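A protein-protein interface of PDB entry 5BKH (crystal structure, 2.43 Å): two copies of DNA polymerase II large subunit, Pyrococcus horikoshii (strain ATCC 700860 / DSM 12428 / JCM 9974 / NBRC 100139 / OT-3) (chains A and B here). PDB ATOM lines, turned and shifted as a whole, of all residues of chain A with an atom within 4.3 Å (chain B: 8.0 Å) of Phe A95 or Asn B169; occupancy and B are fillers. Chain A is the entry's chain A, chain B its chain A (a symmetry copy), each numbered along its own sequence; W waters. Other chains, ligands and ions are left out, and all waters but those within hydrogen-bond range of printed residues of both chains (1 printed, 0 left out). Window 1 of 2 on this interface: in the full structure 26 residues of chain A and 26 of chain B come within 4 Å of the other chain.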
ATOM      1  N   ILE A  85       5.329  13.023  -3.586  1.00  0.00           N
ATOM      2  CA  ILE A  85       5.962  14.257  -3.160  1.00  0.00           C
ATOM      3  C   ILE A  85       5.802  14.358  -1.650  1.00  0.00           C
ATOM      4  O   ILE A  85       4.702  14.145  -1.116  1.00  0.00           O
ATOM      5  CB  ILE A  85       5.342  15.470  -3.870  1.00  0.00           C
ATOM      6  CG1 ILE A  85       6.028  15.712  -5.208  1.00  0.00           C
ATOM      7  CG2 ILE A  85       5.527  16.708  -3.034  1.00  0.00           C
ATOM      8  CD1 ILE A  85       5.399  16.830  -6.007  1.00  0.00           C
ATOM      9  N   ARG A  86       6.897  14.672  -0.962  1.00  0.00           N
ATOM     10  CA  ARG A  86       6.944  14.802   0.487  1.00  0.00           C
ATOM     11  C   ARG A  86       7.274  16.247   0.834  1.00  0.00           C
ATOM     12  O   ARG A  86       8.335  16.757   0.448  1.00  0.00           O
ATOM     13  CB  ARG A  86       7.988  13.861   1.087  1.00  0.00           C
ATOM     14  CG  ARG A  86       7.902  13.726   2.596  1.00  0.00           C
ATOM     15  CD  ARG A  86       8.649  12.498   3.081  1.00  0.00           C
ATOM     16  NE  ARG A  86       9.575  12.821   4.160  1.00  0.00           N
ATOM     17  CZ  ARG A  86       9.229  12.937   5.436  1.00  0.00           C
ATOM     18  NH1 ARG A  86       7.983  12.742   5.836  1.00  0.00           N
ATOM     19  NH2 ARG A  86      10.159  13.250   6.333  1.00  0.00           N
ATOM     20  N   PHE A  87       6.356  16.898   1.543  1.00  0.00           N
ATOM     21  CA  PHE A  87       6.530  18.247   2.059  1.00  0.00           C
ATOM     22  C   PHE A  87       6.883  18.143   3.539  1.00  0.00           C
ATOM     23  O   PHE A  87       6.062  17.698   4.353  1.00  0.00           O
ATOM     24  CB  PHE A  87       5.259  19.072   1.875  1.00  0.00           C
ATOM     25  CG  PHE A  87       4.816  19.214   0.449  1.00  0.00           C
ATOM     26  CD1 PHE A  87       5.540  19.985  -0.442  1.00  0.00           C
ATOM     27  CD2 PHE A  87       3.651  18.602   0.008  1.00  0.00           C
ATOM     28  CE1 PHE A  87       5.123  20.127  -1.755  1.00  0.00           C
ATOM     29  CE2 PHE A  87       3.229  18.743  -1.299  1.00  0.00           C
ATOM     30  CZ  PHE A  87       3.967  19.513  -2.182  1.00  0.00           C
ATOM     31  N   SER A  94       4.539  16.698   8.584  1.00  0.00           N
ATOM     32  CA  SER A  94       4.896  16.143   7.288  1.00  0.00           C
ATOM     33  C   SER A  94       3.644  15.998   6.432  1.00  0.00           C
ATOM     34  O   SER A  94       2.519  15.993   6.937  1.00  0.00           O
ATOM     35  CB  SER A  94       5.583  14.780   7.442  1.00  0.00           C
ATOM     36  OG  SER A  94       6.530  14.563   6.412  1.00  0.00           O
ATOM     37  N   PHE A  95       3.845  15.881   5.119  1.00  0.00           N
ATOM     38  CA  PHE A  95       2.721  15.675   4.204  1.00  0.00           C
ATOM     39  C   PHE A  95       3.222  14.937   2.972  1.00  0.00           C
ATOM     40  O   PHE A  95       3.999  15.494   2.198  1.00  0.00           O
ATOM     41  CB  PHE A  95       2.082  17.011   3.817  1.00  0.00           C
ATOM     42  CG  PHE A  95       0.766  16.879   3.092  1.00  0.00           C
ATOM     43  CD1 PHE A  95      -0.020  15.749   3.242  1.00  0.00           C
ATOM     44  CD2 PHE A  95       0.316  17.894   2.262  1.00  0.00           C
ATOM     45  CE1 PHE A  95      -1.233  15.631   2.577  1.00  0.00           C
ATOM     46  CE2 PHE A  95      -0.894  17.784   1.596  1.00  0.00           C
ATOM     47  CZ  PHE A  95      -1.669  16.652   1.753  1.00  0.00           C
ATOM     48  N   GLU A  96       2.782  13.697   2.780  1.00  0.00           N
ATOM     49  CA  GLU A  96       3.106  12.932   1.582  1.00  0.00           C
ATOM     50  C   GLU A  96       1.859  12.829   0.719  1.00  0.00           C
ATOM     51  O   GLU A  96       0.770  12.540   1.229  1.00  0.00           O
ATOM     52  CB  GLU A  96       3.629  11.538   1.927  1.00  0.00           C
ATOM     53  CG  GLU A  96       5.050  11.522   2.462  1.00  0.00           C
ATOM     54  CD  GLU A  96       5.570  10.117   2.697  1.00  0.00           C
ATOM     55  OE1 GLU A  96       4.887   9.154   2.287  1.00  0.00           O
ATOM     56  OE2 GLU A  96       6.664   9.975   3.284  1.00  0.00           O
ATOM     57  N   THR A  97       2.014  13.067  -0.580  1.00  0.00           N
ATOM     58  CA  THR A  97       0.859  13.086  -1.469  1.00  0.00           C
ATOM     59  C   THR A  97       1.327  12.815  -2.894  1.00  0.00           C
ATOM     60  O   THR A  97       2.519  12.638  -3.156  1.00  0.00           O
ATOM     61  CB  THR A  97       0.111  14.419  -1.356  1.00  0.00           C
ATOM     62  OG1 THR A  97      -1.227  14.262  -1.842  1.00  0.00           O
ATOM     63  CG2 THR A  97       0.827  15.515  -2.144  1.00  0.00           C
ATOM     64  N   VAL A 103      -3.084  20.840  -2.960  1.00  0.00           N
ATOM     65  CA  VAL A 103      -2.638  21.238  -1.633  1.00  0.00           C
ATOM     66  C   VAL A 103      -3.205  22.619  -1.338  1.00  0.00           C
ATOM     67  O   VAL A 103      -3.145  23.517  -2.188  1.00  0.00           O
ATOM     68  CB  VAL A 103      -1.104  21.244  -1.542  1.00  0.00           C
ATOM     69  CG1 VAL A 103      -0.662  21.524  -0.131  1.00  0.00           C
ATOM     70  CG2 VAL A 103      -0.535  19.917  -2.025  1.00  0.00           C
ATOM     71  N   ILE A 127      -2.503  23.727   7.620  1.00  0.00           N
ATOM     72  CA  ILE A 127      -2.732  22.471   8.328  1.00  0.00           C
ATOM     73  C   ILE A 127      -3.720  22.735   9.453  1.00  0.00           C
ATOM     74  O   ILE A 127      -4.158  23.870   9.649  1.00  0.00           O
ATOM     75  CB  ILE A 127      -1.431  21.848   8.867  1.00  0.00           C
ATOM     76  CG1 ILE A 127      -0.921  22.629  10.082  1.00  0.00           C
ATOM     77  CG2 ILE A 127      -0.396  21.697   7.760  1.00  0.00           C
ATOM     78  CD1 ILE A 127       0.441  22.180  10.557  1.00  0.00           C
ATOM     79  N   ARG B  15      -7.741   7.247   8.937  1.00  0.00           N
ATOM     80  CA  ARG B  15      -8.488   7.894  10.009  1.00  0.00           C
ATOM     81  C   ARG B  15      -8.808   9.336   9.640  1.00  0.00           C
ATOM     82  O   ARG B  15      -7.906  10.120   9.329  1.00  0.00           O
ATOM     83  CB  ARG B  15      -7.708   7.859  11.323  1.00  0.00           C
ATOM     84  CG  ARG B  15      -7.127   6.504  11.670  1.00  0.00           C
ATOM     85  CD  ARG B  15      -6.392   6.555  12.995  1.00  0.00           C
ATOM     86  NE  ARG B  15      -7.291   6.276  14.107  1.00  0.00           N
ATOM     87  CZ  ARG B  15      -7.581   5.058  14.542  1.00  0.00           C
ATOM     88  NH1 ARG B  15      -7.059   3.981  13.979  1.00  0.00           N
ATOM     89  NH2 ARG B  15      -8.420   4.918  15.565  1.00  0.00           N
ATOM     90  N   LEU B  17     -11.363  12.850  10.770  1.00  0.00           N
ATOM     91  CA  LEU B  17     -11.828  13.474  11.997  1.00  0.00           C
ATOM     92  C   LEU B  17     -13.260  13.995  11.867  1.00  0.00           C
ATOM     93  O   LEU B  17     -13.603  14.746  10.938  1.00  0.00           O
ATOM     94  CB  LEU B  17     -10.820  14.539  12.447  1.00  0.00           C
ATOM     95  CG  LEU B  17     -11.040  15.662  13.450  1.00  0.00           C
ATOM     96  CD1 LEU B  17      -9.771  15.961  14.169  1.00  0.00           C
ATOM     97  CD2 LEU B  17     -11.263  16.881  12.617  1.00  0.00           C
ATOM     98  N   ARG B  26     -11.156  10.864  15.875  1.00  0.00           N
ATOM     99  CA  ARG B  26     -10.648  10.323  14.625  1.00  0.00           C
ATOM    100  C   ARG B  26     -11.129   8.885  14.477  1.00  0.00           C
ATOM    101  O   ARG B  26     -10.780   8.022  15.290  1.00  0.00           O
ATOM    102  CB  ARG B  26      -9.122  10.402  14.609  1.00  0.00           C
ATOM    103  CG  ARG B  26      -8.586  11.720  15.152  1.00  0.00           C
ATOM    104  CD  ARG B  26      -7.305  12.131  14.448  1.00  0.00           C
ATOM    105  NE  ARG B  26      -6.791  13.405  14.937  1.00  0.00           N
ATOM    106  CZ  ARG B  26      -6.752  14.519  14.219  1.00  0.00           C
ATOM    107  NH1 ARG B  26      -7.151  14.544  12.957  1.00  0.00           N
ATOM    108  NH2 ARG B  26      -6.299  15.636  14.779  1.00  0.00           N
ATOM    109  N   TYR B  58     -15.630  16.758   9.789  1.00  0.00           N
ATOM    110  CA  TYR B  58     -14.929  18.037   9.809  1.00  0.00           C
ATOM    111  C   TYR B  58     -14.290  18.295   8.446  1.00  0.00           C
ATOM    112  O   TYR B  58     -13.484  17.490   7.964  1.00  0.00           O
ATOM    113  CB  TYR B  58     -13.879  18.012  10.913  1.00  0.00           C
ATOM    114  CG  TYR B  58     -14.369  18.414  12.290  1.00  0.00           C
ATOM    115  CD1 TYR B  58     -14.396  17.495  13.342  1.00  0.00           C
ATOM    116  CD2 TYR B  58     -14.671  19.739  12.579  1.00  0.00           C
ATOM    117  CE1 TYR B  58     -14.824  17.862  14.597  1.00  0.00           C
ATOM    118  CE2 TYR B  58     -15.076  20.118  13.851  1.00  0.00           C
ATOM    119  CZ  TYR B  58     -15.144  19.171  14.857  1.00  0.00           C
ATOM    120  OH  TYR B  58     -15.545  19.545  16.123  1.00  0.00           O
ATOM    121  N   THR B 163     -13.645  18.232   1.364  1.00  0.00           N
ATOM    122  CA  THR B 163     -12.321  17.867   1.828  1.00  0.00           C
ATOM    123  C   THR B 163     -12.412  17.219   3.206  1.00  0.00           C
ATOM    124  O   THR B 163     -13.424  17.321   3.906  1.00  0.00           O
ATOM    125  CB  THR B 163     -11.412  19.093   1.864  1.00  0.00           C
ATOM    126  OG1 THR B 163     -10.050  18.672   1.741  1.00  0.00           O
ATOM    127  CG2 THR B 163     -11.590  19.850   3.164  1.00  0.00           C
ATOM    128  N   VAL B 164     -11.336  16.543   3.593  1.00  0.00           N
ATOM    129  CA  VAL B 164     -11.333  15.734   4.802  1.00  0.00           C
ATOM    130  C   VAL B 164     -10.023  15.957   5.547  1.00  0.00           C
ATOM    131  O   VAL B 164      -8.982  16.233   4.944  1.00  0.00           O
ATOM    132  CB  VAL B 164     -11.571  14.244   4.449  1.00  0.00           C
ATOM    133  CG1 VAL B 164     -10.440  13.361   4.917  1.00  0.00           C
ATOM    134  CG2 VAL B 164     -12.890  13.779   5.029  1.00  0.00           C
ATOM    135  N   ILE B 165     -10.079  15.856   6.871  1.00  0.00           N
ATOM    136  CA  ILE B 165      -8.942  16.178   7.724  1.00  0.00           C
ATOM    137  C   ILE B 165      -8.336  14.877   8.228  1.00  0.00           C
ATOM    138  O   ILE B 165      -8.920  14.182   9.067  1.00  0.00           O
ATOM    139  CB  ILE B 165      -9.346  17.098   8.881  1.00  0.00           C
ATOM    140  CG1 ILE B 165      -9.876  18.419   8.319  1.00  0.00           C
ATOM    141  CG2 ILE B 165      -8.158  17.346   9.798  1.00  0.00           C
ATOM    142  CD1 ILE B 165     -10.885  19.095   9.202  1.00  0.00           C
ATOM    143  N   ILE B 166      -7.151  14.563   7.718  1.00  0.00           N
ATOM    144  CA  ILE B 166      -6.433  13.339   8.045  1.00  0.00           C
ATOM    145  C   ILE B 166      -5.199  13.747   8.835  1.00  0.00           C
ATOM    146  O   ILE B 166      -4.313  14.422   8.297  1.00  0.00           O
ATOM    147  CB  ILE B 166      -6.038  12.565   6.779  1.00  0.00           C
ATOM    148  CG1 ILE B 166      -7.282  12.200   5.968  1.00  0.00           C
ATOM    149  CG2 ILE B 166      -5.238  11.327   7.149  1.00  0.00           C
ATOM    150  CD1 ILE B 166      -7.019  11.241   4.830  1.00  0.00           C
ATOM    151  N   ASN B 167      -5.138  13.327  10.100  1.00  0.00           N
ATOM    152  CA  ASN B 167      -4.112  13.799  11.025  1.00  0.00           C
ATOM    153  C   ASN B 167      -4.152  15.319  11.091  1.00  0.00           C
ATOM    154  O   ASN B 167      -5.125  15.898  11.584  1.00  0.00           O
ATOM    155  CB  ASN B 167      -2.720  13.312  10.611  1.00  0.00           C
ATOM    156  CG  ASN B 167      -2.563  11.812  10.747  1.00  0.00           C
ATOM    157  OD1 ASN B 167      -3.177  11.187  11.612  1.00  0.00           O
ATOM    158  ND2 ASN B 167      -1.742  11.225   9.881  1.00  0.00           N
ATOM    159  N   GLU B 168      -3.111  15.972  10.575  1.00  0.00           N
ATOM    160  CA  GLU B 168      -3.040  17.426  10.557  1.00  0.00           C
ATOM    161  C   GLU B 168      -3.359  18.019   9.191  1.00  0.00           C
ATOM    162  O   GLU B 168      -3.479  19.244   9.078  1.00  0.00           O
ATOM    163  CB  GLU B 168      -1.644  17.889  10.996  1.00  0.00           C
ATOM    164  CG  GLU B 168      -1.265  17.473  12.412  1.00  0.00           C
ATOM    165  CD  GLU B 168      -0.424  18.514  13.135  1.00  0.00           C
ATOM    166  OE1 GLU B 168       0.706  18.783  12.677  1.00  0.00           O
ATOM    167  OE2 GLU B 168      -0.884  19.049  14.167  1.00  0.00           O
ATOM    168  N   ASN B 169      -3.515  17.190   8.166  1.00  0.00           N
ATOM    169  CA  ASN B 169      -3.565  17.653   6.789  1.00  0.00           C
ATOM    170  C   ASN B 169      -4.992  17.719   6.255  1.00  0.00           C
ATOM    171  O   ASN B 169      -5.886  16.998   6.703  1.00  0.00           O
ATOM    172  CB  ASN B 169      -2.723  16.746   5.892  1.00  0.00           C
ATOM    173  CG  ASN B 169      -1.247  16.802   6.234  1.00  0.00           C
ATOM    174  OD1 ASN B 169      -0.637  15.791   6.578  1.00  0.00           O
ATOM    175  ND2 ASN B 169      -0.665  17.993   6.141  1.00  0.00           N
ATOM    176  N   ILE B 170      -5.178  18.595   5.275  1.00  0.00           N
ATOM    177  CA  ILE B 170      -6.443  18.778   4.574  1.00  0.00           C
ATOM    178  C   ILE B 170      -6.298  18.079   3.226  1.00  0.00           C
ATOM    179  O   ILE B 170      -5.646  18.598   2.318  1.00  0.00           O
ATOM    180  CB  ILE B 170      -6.776  20.263   4.409  1.00  0.00           C
ATOM    181  CG1 ILE B 170      -6.766  20.977   5.762  1.00  0.00           C
ATOM    182  CG2 ILE B 170      -8.103  20.451   3.694  1.00  0.00           C
ATOM    183  CD1 ILE B 170      -6.863  22.492   5.650  1.00  0.00           C
ATOM    184  N   VAL B 171      -6.899  16.899   3.081  1.00  0.00           N
ATOM    185  CA  VAL B 171      -6.732  16.101   1.872  1.00  0.00           C
ATOM    186  C   VAL B 171      -8.073  15.967   1.160  1.00  0.00           C
ATOM    187  O   VAL B 171      -9.141  15.940   1.782  1.00  0.00           O
ATOM    188  CB  VAL B 171      -6.106  14.720   2.177  1.00  0.00           C
ATOM    189  CG1 VAL B 171      -5.638  14.656   3.617  1.00  0.00           C
ATOM    190  CG2 VAL B 171      -7.068  13.586   1.869  1.00  0.00           C
ATOM    191  N   THR B 172      -8.006  15.920  -0.169  1.00  0.00           N
ATOM    192  CA  THR B 172      -9.188  15.753  -1.001  1.00  0.00           C
ATOM    193  C   THR B 172      -9.519  14.283  -1.232  1.00  0.00           C
ATOM    194  O   THR B 172     -10.691  13.891  -1.161  1.00  0.00           O
ATOM    195  CB  THR B 172      -8.989  16.466  -2.345  1.00  0.00           C
ATOM    196  OG1 THR B 172      -8.859  17.878  -2.126  1.00  0.00           O
ATOM    197  CG2 THR B 172     -10.169  16.215  -3.265  1.00  0.00           C
ATOM    198  N   HIS B 173      -8.510  13.456  -1.488  1.00  0.00           N
ATOM    199  CA  HIS B 173      -8.730  12.045  -1.770  1.00  0.00           C
ATOM    200  C   HIS B 173      -7.416  11.302  -1.578  1.00  0.00           C
ATOM    201  O   HIS B 173      -6.379  11.897  -1.272  1.00  0.00           O
ATOM    202  CB  HIS B 173      -9.271  11.838  -3.186  1.00  0.00           C
ATOM    203  CG  HIS B 173      -8.417  12.457  -4.247  1.00  0.00           C
ATOM    204  ND1 HIS B 173      -8.829  13.537  -4.998  1.00  0.00           N
ATOM    205  CD2 HIS B 173      -7.170  12.153  -4.680  1.00  0.00           C
ATOM    206  CE1 HIS B 173      -7.874  13.872  -5.845  1.00  0.00           C
ATOM    207  NE2 HIS B 173      -6.856  13.048  -5.673  1.00  0.00           N
ATOM    208  N   GLN B 174      -7.470   9.989  -1.779  1.00  0.00           N
ATOM    209  CA  GLN B 174      -6.293   9.129  -1.744  1.00  0.00           C
ATOM    210  C   GLN B 174      -6.386   8.080  -2.845  1.00  0.00           C
ATOM    211  O   GLN B 174      -6.070   6.902  -2.638  1.00  0.00           O
ATOM    212  CB  GLN B 174      -6.127   8.479  -0.370  1.00  0.00           C
ATOM    213  CG  GLN B 174      -5.011   9.090   0.469  1.00  0.00           C
ATOM    214  CD  GLN B 174      -5.153   8.798   1.954  1.00  0.00           C
ATOM    215  OE1 GLN B 174      -6.011   8.018   2.370  1.00  0.00           O
ATOM    216  NE2 GLN B 174      -4.300   9.425   2.763  1.00  0.00           N
HETATM  217  O   HOH W   1      -2.305  11.897   1.954  1.00  0.00           O
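The side-chain amide oxygen (OD1) of Asn B169 lies close to the backbone carbonyl oxygen (O) of Ser A94 (3.2 Å).
Among the printed residues, pairs that only touch across the chains: Phe A95 with Asn B169 and Ile A127 with Glu B168.
No position is printed for both chains.
Of the 9 printed residues of chain A, 3 touch a printed residue of chain B.
Printed residues of chain A that touch a printed residue of chain B: Ser A94, Phe A95 and Ile A127.
Hydrophobic or aromatic side chains of chain A that line the printed part of chain B: Phe A95 and Ile A127.
Water W1 bridges the backbone carbonyl oxygen (O) of Glu A96 (3.2 Å) and the side-chain amide nitrogen (NE2) of Gln B174 (3.3 Å).
N of Phe A87 is in hydrogen-bond range of O of Phe A95 (2.8 Å).
Phe A95 touches just one residue of chain B: Asn B169 (3.4 Å).
Of chain A, only Ser A94 and Phe A95 come within 4 Å of Asn B169.
Of chain B, only Asn B169 (3.2 Å) comes within 4 Å of Ser A94.
Of the printed residues of chain A, Glu B168 touches Ile A127 (3.3 Å).
Of the printed residues of chain B, Ile A127 touches Glu B168 (3.3 Å).
Ile B166 touches none of the printed residues of chain A.
The nearest residue of chain B that does not touch Phe A95 is Ile B170 (4.5 Å).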
